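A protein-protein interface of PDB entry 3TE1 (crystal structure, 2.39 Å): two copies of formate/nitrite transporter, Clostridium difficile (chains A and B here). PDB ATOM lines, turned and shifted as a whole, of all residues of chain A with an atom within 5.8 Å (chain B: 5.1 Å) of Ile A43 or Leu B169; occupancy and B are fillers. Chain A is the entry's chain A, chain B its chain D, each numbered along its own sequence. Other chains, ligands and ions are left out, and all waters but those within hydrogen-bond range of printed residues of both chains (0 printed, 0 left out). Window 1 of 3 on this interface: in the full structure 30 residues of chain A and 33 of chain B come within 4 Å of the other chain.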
ATOM      1  N   GLY A  38     -10.251  10.979   6.966  1.00  0.00           N
ATOM      2  CA  GLY A  38     -11.370  10.979   7.890  1.00  0.00           C
ATOM      3  C   GLY A  38     -10.930  10.613   9.295  1.00  0.00           C
ATOM      4  O   GLY A  38     -11.337  11.256  10.266  1.00  0.00           O
ATOM      5  N   LEU A  39     -10.076   9.598   9.413  1.00  0.00           N
ATOM      6  CA  LEU A  39      -9.577   9.148  10.715  1.00  0.00           C
ATOM      7  C   LEU A  39      -8.486  10.071  11.314  1.00  0.00           C
ATOM      8  O   LEU A  39      -8.446  10.343  12.528  1.00  0.00           O
ATOM      9  CB  LEU A  39      -9.097   7.699  10.585  1.00  0.00           C
ATOM     10  CG  LEU A  39      -8.628   6.895  11.791  1.00  0.00           C
ATOM     11  CD1 LEU A  39      -8.849   5.348  11.506  1.00  0.00           C
ATOM     12  CD2 LEU A  39      -7.158   7.226  12.069  1.00  0.00           C
ATOM     13  N   TYR A  40      -7.596  10.552  10.455  1.00  0.00           N
ATOM     14  CA  TYR A  40      -6.624  11.590  10.837  1.00  0.00           C
ATOM     15  C   TYR A  40      -7.288  12.824  11.373  1.00  0.00           C
ATOM     16  O   TYR A  40      -6.859  13.351  12.385  1.00  0.00           O
ATOM     17  CB  TYR A  40      -5.754  11.981   9.639  1.00  0.00           C
ATOM     18  CG  TYR A  40      -4.799  10.885   9.262  1.00  0.00           C
ATOM     19  CD1 TYR A  40      -4.338  10.002  10.234  1.00  0.00           C
ATOM     20  CD2 TYR A  40      -4.384  10.708   7.953  1.00  0.00           C
ATOM     21  CE1 TYR A  40      -3.485   8.998   9.924  1.00  0.00           C
ATOM     22  CE2 TYR A  40      -3.511   9.693   7.632  1.00  0.00           C
ATOM     23  CZ  TYR A  40      -3.060   8.847   8.623  1.00  0.00           C
ATOM     24  OH  TYR A  40      -2.196   7.828   8.333  1.00  0.00           O
ATOM     25  N   VAL A  41      -8.346  13.272  10.703  1.00  0.00           N
ATOM     26  CA  VAL A  41      -9.121  14.426  11.169  1.00  0.00           C
ATOM     27  C   VAL A  41      -9.772  14.137  12.512  1.00  0.00           C
ATOM     28  O   VAL A  41      -9.784  15.000  13.415  1.00  0.00           O
ATOM     29  CB  VAL A  41     -10.184  14.841  10.136  1.00  0.00           C
ATOM     30  CG1 VAL A  41     -11.180  15.767  10.758  1.00  0.00           C
ATOM     31  CG2 VAL A  41      -9.514  15.512   8.918  1.00  0.00           C
ATOM     32  N   GLY A  42     -10.281  12.906  12.646  1.00  0.00           N
ATOM     33  CA  GLY A  42     -11.027  12.489  13.823  1.00  0.00           C
ATOM     34  C   GLY A  42     -10.141  12.515  15.050  1.00  0.00           C
ATOM     35  O   GLY A  42     -10.572  12.911  16.150  1.00  0.00           O
ATOM     36  N   ILE A  43      -8.885  12.121  14.868  1.00  0.00           N
ATOM     37  CA  ILE A  43      -7.912  12.200  15.963  1.00  0.00           C
ATOM     38  C   ILE A  43      -7.904  13.569  16.648  1.00  0.00           C
ATOM     39  O   ILE A  43      -8.014  13.652  17.880  1.00  0.00           O
ATOM     40  CB  ILE A  43      -6.482  11.815  15.486  1.00  0.00           C
ATOM     41  CG1 ILE A  43      -6.417  10.305  15.206  1.00  0.00           C
ATOM     42  CG2 ILE A  43      -5.379  12.291  16.490  1.00  0.00           C
ATOM     43  CD1 ILE A  43      -4.991   9.768  14.811  1.00  0.00           C
ATOM     44  N   GLY A  44      -7.767  14.649  15.872  1.00  0.00           N
ATOM     45  CA  GLY A  44      -7.862  15.986  16.470  1.00  0.00           C
ATOM     46  C   GLY A  44      -9.183  16.227  17.220  1.00  0.00           C
ATOM     47  O   GLY A  44      -9.182  16.757  18.331  1.00  0.00           O
ATOM     48  N   ILE A  45     -10.322  15.846  16.623  1.00  0.00           N
ATOM     49  CA  ILE A  45     -11.580  15.828  17.412  1.00  0.00           C
ATOM     50  C   ILE A  45     -11.408  15.107  18.775  1.00  0.00           C
ATOM     51  O   ILE A  45     -11.837  15.637  19.814  1.00  0.00           O
ATOM     52  CB  ILE A  45     -12.808  15.235  16.617  1.00  0.00           C
ATOM     53  CG1 ILE A  45     -13.437  16.234  15.621  1.00  0.00           C
ATOM     54  CG2 ILE A  45     -13.798  14.544  17.526  1.00  0.00           C
ATOM     55  CD1 ILE A  45     -13.337  17.711  15.961  1.00  0.00           C
ATOM     56  N   LEU A  46     -10.777  13.926  18.795  1.00  0.00           N
ATOM     57  CA  LEU A  46     -10.604  13.199  20.069  1.00  0.00           C
ATOM     58  C   LEU A  46      -9.780  14.007  21.057  1.00  0.00           C
ATOM     59  O   LEU A  46     -10.173  14.170  22.234  1.00  0.00           O
ATOM     60  CB  LEU A  46      -9.959  11.819  19.875  1.00  0.00           C
ATOM     61  CG  LEU A  46     -10.748  10.898  18.942  1.00  0.00           C
ATOM     62  CD1 LEU A  46     -10.011   9.557  18.633  1.00  0.00           C
ATOM     63  CD2 LEU A  46     -12.126  10.669  19.540  1.00  0.00           C
ATOM     64  N   LEU A  47      -8.639  14.498  20.570  1.00  0.00           N
ATOM     65  CA  LEU A  47      -7.726  15.313  21.390  1.00  0.00           C
ATOM     66  C   LEU A  47      -8.373  16.609  21.856  1.00  0.00           C
ATOM     67  O   LEU A  47      -8.292  16.966  23.047  1.00  0.00           O
ATOM     68  CB  LEU A  47      -6.448  15.686  20.631  1.00  0.00           C
ATOM     69  CG  LEU A  47      -5.644  16.782  21.319  1.00  0.00           C
ATOM     70  CD1 LEU A  47      -5.171  16.261  22.711  1.00  0.00           C
ATOM     71  CD2 LEU A  47      -4.451  17.216  20.438  1.00  0.00           C
ATOM     72  N   ILE A  48      -9.002  17.329  20.927  1.00  0.00           N
ATOM     73  CA  ILE A  48      -9.577  18.587  21.360  1.00  0.00           C
ATOM     74  C   ILE A  48     -10.836  18.405  22.273  1.00  0.00           C
ATOM     75  O   ILE A  48     -10.988  19.139  23.247  1.00  0.00           O
ATOM     76  CB  ILE A  48      -9.745  19.655  20.244  1.00  0.00           C
ATOM     77  CG1 ILE A  48     -10.886  19.323  19.239  1.00  0.00           C
ATOM     78  CG2 ILE A  48      -8.382  20.054  19.661  1.00  0.00           C
ATOM     79  CD1 ILE A  48     -11.471  20.678  18.558  1.00  0.00           C
ATOM     80  N   ILE A  73      -3.084  19.073  14.308  1.00  0.00           N
ATOM     81  CA  ILE A  73      -2.837  17.693  13.909  1.00  0.00           C
ATOM     82  C   ILE A  73      -3.743  17.180  12.790  1.00  0.00           C
ATOM     83  O   ILE A  73      -3.287  16.407  11.913  1.00  0.00           O
ATOM     84  CB  ILE A  73      -2.793  16.724  15.131  1.00  0.00           C
ATOM     85  CG1 ILE A  73      -2.238  15.351  14.715  1.00  0.00           C
ATOM     86  CG2 ILE A  73      -4.144  16.617  15.842  1.00  0.00           C
ATOM     87  CD1 ILE A  73      -1.734  14.546  15.880  1.00  0.00           C
ATOM     88  N   LEU A  77      -1.767  15.905   9.692  1.00  0.00           N
ATOM     89  CA  LEU A  77      -1.590  14.503   9.314  1.00  0.00           C
ATOM     90  C   LEU A  77      -1.981  14.369   7.854  1.00  0.00           C
ATOM     91  O   LEU A  77      -1.141  14.012   7.017  1.00  0.00           O
ATOM     92  CB  LEU A  77      -2.370  13.537  10.226  1.00  0.00           C
ATOM     93  CG  LEU A  77      -1.870  13.331  11.679  1.00  0.00           C
ATOM     94  CD1 LEU A  77      -2.846  12.446  12.490  1.00  0.00           C
ATOM     95  CD2 LEU A  77      -0.447  12.737  11.725  1.00  0.00           C
ATOM     96  N   LEU A 125     -12.900   5.169  13.722  1.00  0.00           N
ATOM     97  CA  LEU A 125     -12.266   5.809  14.866  1.00  0.00           C
ATOM     98  C   LEU A 125     -13.245   5.818  16.057  1.00  0.00           C
ATOM     99  O   LEU A 125     -12.850   5.581  17.213  1.00  0.00           O
ATOM    100  CB  LEU A 125     -11.838   7.250  14.510  1.00  0.00           C
ATOM    101  CG  LEU A 125     -11.023   7.934  15.611  1.00  0.00           C
ATOM    102  CD1 LEU A 125      -9.669   7.211  15.790  1.00  0.00           C
ATOM    103  CD2 LEU A 125     -10.808   9.466  15.371  1.00  0.00           C
ATOM    104  N   THR A 210     -16.805  12.437  13.003  1.00  0.00           N
ATOM    105  CA  THR A 210     -16.250  11.761  14.179  1.00  0.00           C
ATOM    106  C   THR A 210     -17.050  12.036  15.460  1.00  0.00           C
ATOM    107  O   THR A 210     -17.331  11.115  16.223  1.00  0.00           O
ATOM    108  CB  THR A 210     -14.721  11.993  14.338  1.00  0.00           C
ATOM    109  OG1 THR A 210     -14.058  11.323  13.263  1.00  0.00           O
ATOM    110  CG2 THR A 210     -14.172  11.429  15.678  1.00  0.00           C
ATOM    111  N   ILE B 164      -4.105   0.325  20.374  1.00  0.00           N
ATOM    112  CA  ILE B 164      -4.317   0.537  18.935  1.00  0.00           C
ATOM    113  C   ILE B 164      -4.231   2.024  18.576  1.00  0.00           C
ATOM    114  O   ILE B 164      -3.388   2.438  17.775  1.00  0.00           O
ATOM    115  CB  ILE B 164      -5.703   0.046  18.531  1.00  0.00           C
ATOM    116  CG1 ILE B 164      -5.754  -1.498  18.698  1.00  0.00           C
ATOM    117  CG2 ILE B 164      -6.050   0.524  17.125  1.00  0.00           C
ATOM    118  CD1 ILE B 164      -7.106  -2.173  18.450  1.00  0.00           C
ATOM    119  N   LEU B 165      -5.100   2.832  19.192  1.00  0.00           N
ATOM    120  CA  LEU B 165      -5.082   4.263  18.945  1.00  0.00           C
ATOM    121  C   LEU B 165      -3.664   4.827  19.178  1.00  0.00           C
ATOM    122  O   LEU B 165      -3.141   5.608  18.362  1.00  0.00           O
ATOM    123  CB  LEU B 165      -6.182   4.986  19.760  1.00  0.00           C
ATOM    124  CG  LEU B 165      -7.589   4.722  19.162  1.00  0.00           C
ATOM    125  CD1 LEU B 165      -8.675   5.689  19.631  1.00  0.00           C
ATOM    126  CD2 LEU B 165      -7.540   4.734  17.618  1.00  0.00           C
ATOM    127  N   CYS B 166      -3.007   4.386  20.246  1.00  0.00           N
ATOM    128  CA  CYS B 166      -1.658   4.858  20.506  1.00  0.00           C
ATOM    129  C   CYS B 166      -0.664   4.607  19.355  1.00  0.00           C
ATOM    130  O   CYS B 166      -0.016   5.539  18.861  1.00  0.00           O
ATOM    131  CB  CYS B 166      -1.123   4.243  21.782  1.00  0.00           C
ATOM    132  SG  CYS B 166       0.603   4.717  21.997  1.00  0.00           S
ATOM    133  N   ASN B 167      -0.526   3.352  18.938  1.00  0.00           N
ATOM    134  CA  ASN B 167       0.409   3.055  17.870  1.00  0.00           C
ATOM    135  C   ASN B 167      -0.011   3.537  16.477  1.00  0.00           C
ATOM    136  O   ASN B 167       0.846   3.633  15.563  1.00  0.00           O
ATOM    137  CB  ASN B 167       0.837   1.576  17.835  1.00  0.00           C
ATOM    138  CG  ASN B 167       2.228   1.404  17.225  1.00  0.00           C
ATOM    139  OD1 ASN B 167       3.024   2.350  17.239  1.00  0.00           O
ATOM    140  ND2 ASN B 167       2.514   0.227  16.665  1.00  0.00           N
ATOM    141  N   ILE B 168      -1.298   3.865  16.297  1.00  0.00           N
ATOM    142  CA  ILE B 168      -1.669   4.560  15.053  1.00  0.00           C
ATOM    143  C   ILE B 168      -0.979   5.941  15.073  1.00  0.00           C
ATOM    144  O   ILE B 168      -0.426   6.402  14.074  1.00  0.00           O
ATOM    145  CB  ILE B 168      -3.188   4.770  14.861  1.00  0.00           C
ATOM    146  CG1 ILE B 168      -3.889   3.451  14.557  1.00  0.00           C
ATOM    147  CG2 ILE B 168      -3.432   5.774  13.733  1.00  0.00           C
ATOM    148  CD1 ILE B 168      -5.404   3.599  14.433  1.00  0.00           C
ATOM    149  N   LEU B 169      -0.989   6.578  16.237  1.00  0.00           N
ATOM    150  CA  LEU B 169      -0.384   7.884  16.372  1.00  0.00           C
ATOM    151  C   LEU B 169       1.155   7.808  16.315  1.00  0.00           C
ATOM    152  O   LEU B 169       1.800   8.612  15.631  1.00  0.00           O
ATOM    153  CB  LEU B 169      -0.880   8.547  17.647  1.00  0.00           C
ATOM    154  CG  LEU B 169      -2.161   9.328  17.363  1.00  0.00           C
ATOM    155  CD1 LEU B 169      -2.830   9.660  18.676  1.00  0.00           C
ATOM    156  CD2 LEU B 169      -1.828  10.599  16.568  1.00  0.00           C
ATOM    157  N   VAL B 170       1.747   6.848  17.019  1.00  0.00           N
ATOM    158  CA  VAL B 170       3.207   6.734  17.015  1.00  0.00           C
ATOM    159  C   VAL B 170       3.690   6.408  15.605  1.00  0.00           C
ATOM    160  O   VAL B 170       4.548   7.105  15.047  1.00  0.00           O
ATOM    161  CB  VAL B 170       3.720   5.715  18.046  1.00  0.00           C
ATOM    162  CG1 VAL B 170       5.128   5.272  17.681  1.00  0.00           C
ATOM    163  CG2 VAL B 170       3.651   6.323  19.460  1.00  0.00           C
ATOM    164  N   CYS B 171       3.052   5.412  15.007  1.00  0.00           N
ATOM    165  CA  CYS B 171       3.380   4.998  13.646  1.00  0.00           C
ATOM    166  C   CYS B 171       3.151   6.023  12.526  1.00  0.00           C
ATOM    167  O   CYS B 171       3.955   6.104  11.610  1.00  0.00           O
ATOM    168  CB  CYS B 171       2.691   3.679  13.303  1.00  0.00           C
ATOM    169  SG  CYS B 171       3.587   2.287  13.992  1.00  0.00           S
ATOM    170  N   VAL B 172       2.069   6.789  12.586  1.00  0.00           N
ATOM    171  CA  VAL B 172       1.806   7.749  11.526  1.00  0.00           C
ATOM    172  C   VAL B 172       2.845   8.844  11.664  1.00  0.00           C
ATOM    173  O   VAL B 172       3.191   9.494  10.691  1.00  0.00           O
ATOM    174  CB  VAL B 172       0.350   8.323  11.554  1.00  0.00           C
ATOM    175  CG1 VAL B 172       0.138   9.255  12.748  1.00  0.00           C
ATOM    176  CG2 VAL B 172       0.041   9.038  10.253  1.00  0.00           C
ATOM    177  N   SER B 173       3.362   9.012  12.879  1.00  0.00           N
ATOM    178  CA  SER B 173       4.415   9.994  13.112  1.00  0.00           C
ATOM    179  C   SER B 173       5.799   9.482  12.629  1.00  0.00           C
ATOM    180  O   SER B 173       6.624  10.270  12.153  1.00  0.00           O
ATOM    181  CB  SER B 173       4.416  10.460  14.578  1.00  0.00           C
ATOM    182  OG  SER B 173       5.434   9.807  15.315  1.00  0.00           O
ATOM    183  N   CYS B 193       1.710  14.371  17.306  1.00  0.00           N
ATOM    184  CA  CYS B 193       1.160  13.040  17.466  1.00  0.00           C
ATOM    185  C   CYS B 193       1.268  12.584  18.915  1.00  0.00           C
ATOM    186  O   CYS B 193       0.329  11.995  19.421  1.00  0.00           O
ATOM    187  CB  CYS B 193       1.841  12.055  16.536  1.00  0.00           C
ATOM    188  SG  CYS B 193       1.413  12.345  14.861  1.00  0.00           S
ATOM    189  N   ALA B 196      -1.223  14.333  21.095  1.00  0.00           N
ATOM    190  CA  ALA B 196      -2.542  13.779  20.875  1.00  0.00           C
ATOM    191  C   ALA B 196      -2.686  12.446  21.605  1.00  0.00           C
ATOM    192  O   ALA B 196      -3.718  12.194  22.256  1.00  0.00           O
ATOM    193  CB  ALA B 196      -2.797  13.588  19.378  1.00  0.00           C
ATOM    194  N   PHE B 197      -1.669  11.580  21.510  1.00  0.00           N
ATOM    195  CA  PHE B 197      -1.861  10.251  22.104  1.00  0.00           C
ATOM    196  C   PHE B 197      -1.775  10.283  23.662  1.00  0.00           C
ATOM    197  O   PHE B 197      -2.604   9.676  24.354  1.00  0.00           O
ATOM    198  CB  PHE B 197      -0.995   9.149  21.417  1.00  0.00           C
ATOM    199  CG  PHE B 197       0.183   8.694  22.238  1.00  0.00           C
ATOM    200  CD1 PHE B 197      -0.005   8.114  23.497  1.00  0.00           C
ATOM    201  CD2 PHE B 197       1.480   8.859  21.770  1.00  0.00           C
ATOM    202  CE1 PHE B 197       1.077   7.701  24.284  1.00  0.00           C
ATOM    203  CE2 PHE B 197       2.565   8.439  22.557  1.00  0.00           C
ATOM    204  CZ  PHE B 197       2.353   7.863  23.812  1.00  0.00           C
ATOM    205  N   PHE B 202      -4.212   7.449  25.482  1.00  0.00           N
ATOM    206  CA  PHE B 202      -3.832   6.198  24.830  1.00  0.00           C
ATOM    207  C   PHE B 202      -2.642   5.516  25.473  1.00  0.00           C
ATOM    208  O   PHE B 202      -1.867   6.142  26.193  1.00  0.00           O
ATOM    209  CB  PHE B 202      -3.602   6.405  23.344  1.00  0.00           C
ATOM    210  CG  PHE B 202      -4.759   7.038  22.679  1.00  0.00           C
ATOM    211  CD1 PHE B 202      -6.033   6.719  23.099  1.00  0.00           C
ATOM    212  CD2 PHE B 202      -4.587   7.997  21.680  1.00  0.00           C
ATOM    213  CE1 PHE B 202      -7.149   7.329  22.519  1.00  0.00           C
ATOM    214  CE2 PHE B 202      -5.697   8.616  21.091  1.00  0.00           C
ATOM    215  CZ  PHE B 202      -6.976   8.280  21.508  1.00  0.00           C
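Val B172 touches Tyr A40 (CG2 to OH, 3.2 Å). CD1 of Ile A43 touches CD2 of Leu B169, at 3.7 Å. Ala B196 touches Leu A47. Ile A73 touches Cys B193 (CD1 to CA, 3.6 Å). Ile A73 touches Ala B196 (CD1 to CB, 3.8 Å). Leu A77 touches Val B172. Leu A77 touches Cys B193. Leu A125 touches Leu B165 (CD1 to CD2, 3.7 Å).
Of the printed residues of chain B, Tyr A40 touches Val B172 (3.2 Å). Ile A43 touches just one residue of chain B: Leu B169 (3.7 Å). Of the printed residues of chain B, Leu A77 touches Val B172 and Cys B193. Of the printed residues of chain A, Leu B165 touches Leu A125. Printed residues of chain A within 4 Å of Leu B169: Ile A43 (3.7 Å). The nearest residue of chain B that does not touch Ile A43 is Ala B196 (4.1 Å). The nearest printed residue of chain A that does not touch Leu B169 is Ile A73 (4.01 Å). The nearest printed residue of chain B that does not touch Leu A125 is Ile B168 (5.8 Å).
Of the 14 printed residues of chain B, 5 touch a printed residue of chain A. Printed residues of chain B that touch a printed residue of chain A: Leu B165, Leu B169, Val B172, Cys B193 and Ala B196. Hydrophobic or aromatic side chains of chain B that line the printed part of chain A: Leu B165, Leu B169, Val B172 and Ala B196. Hydrophobic or aromatic side chains of chain A within 4 Å of the printed part of chain B: Tyr A40, Ile A43, Leu A47, Ile A73, Leu A77 and Leu A125. Among the printed residues, no Asp or Glu carboxylate lies within 4 Å of a Lys or Arg side-chain nitrogen of the other chain.
No position is printed for both chains. Of the 8 pairs that touch across the chains among the printed residues, none has its exchanged pair printed and touching as well.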
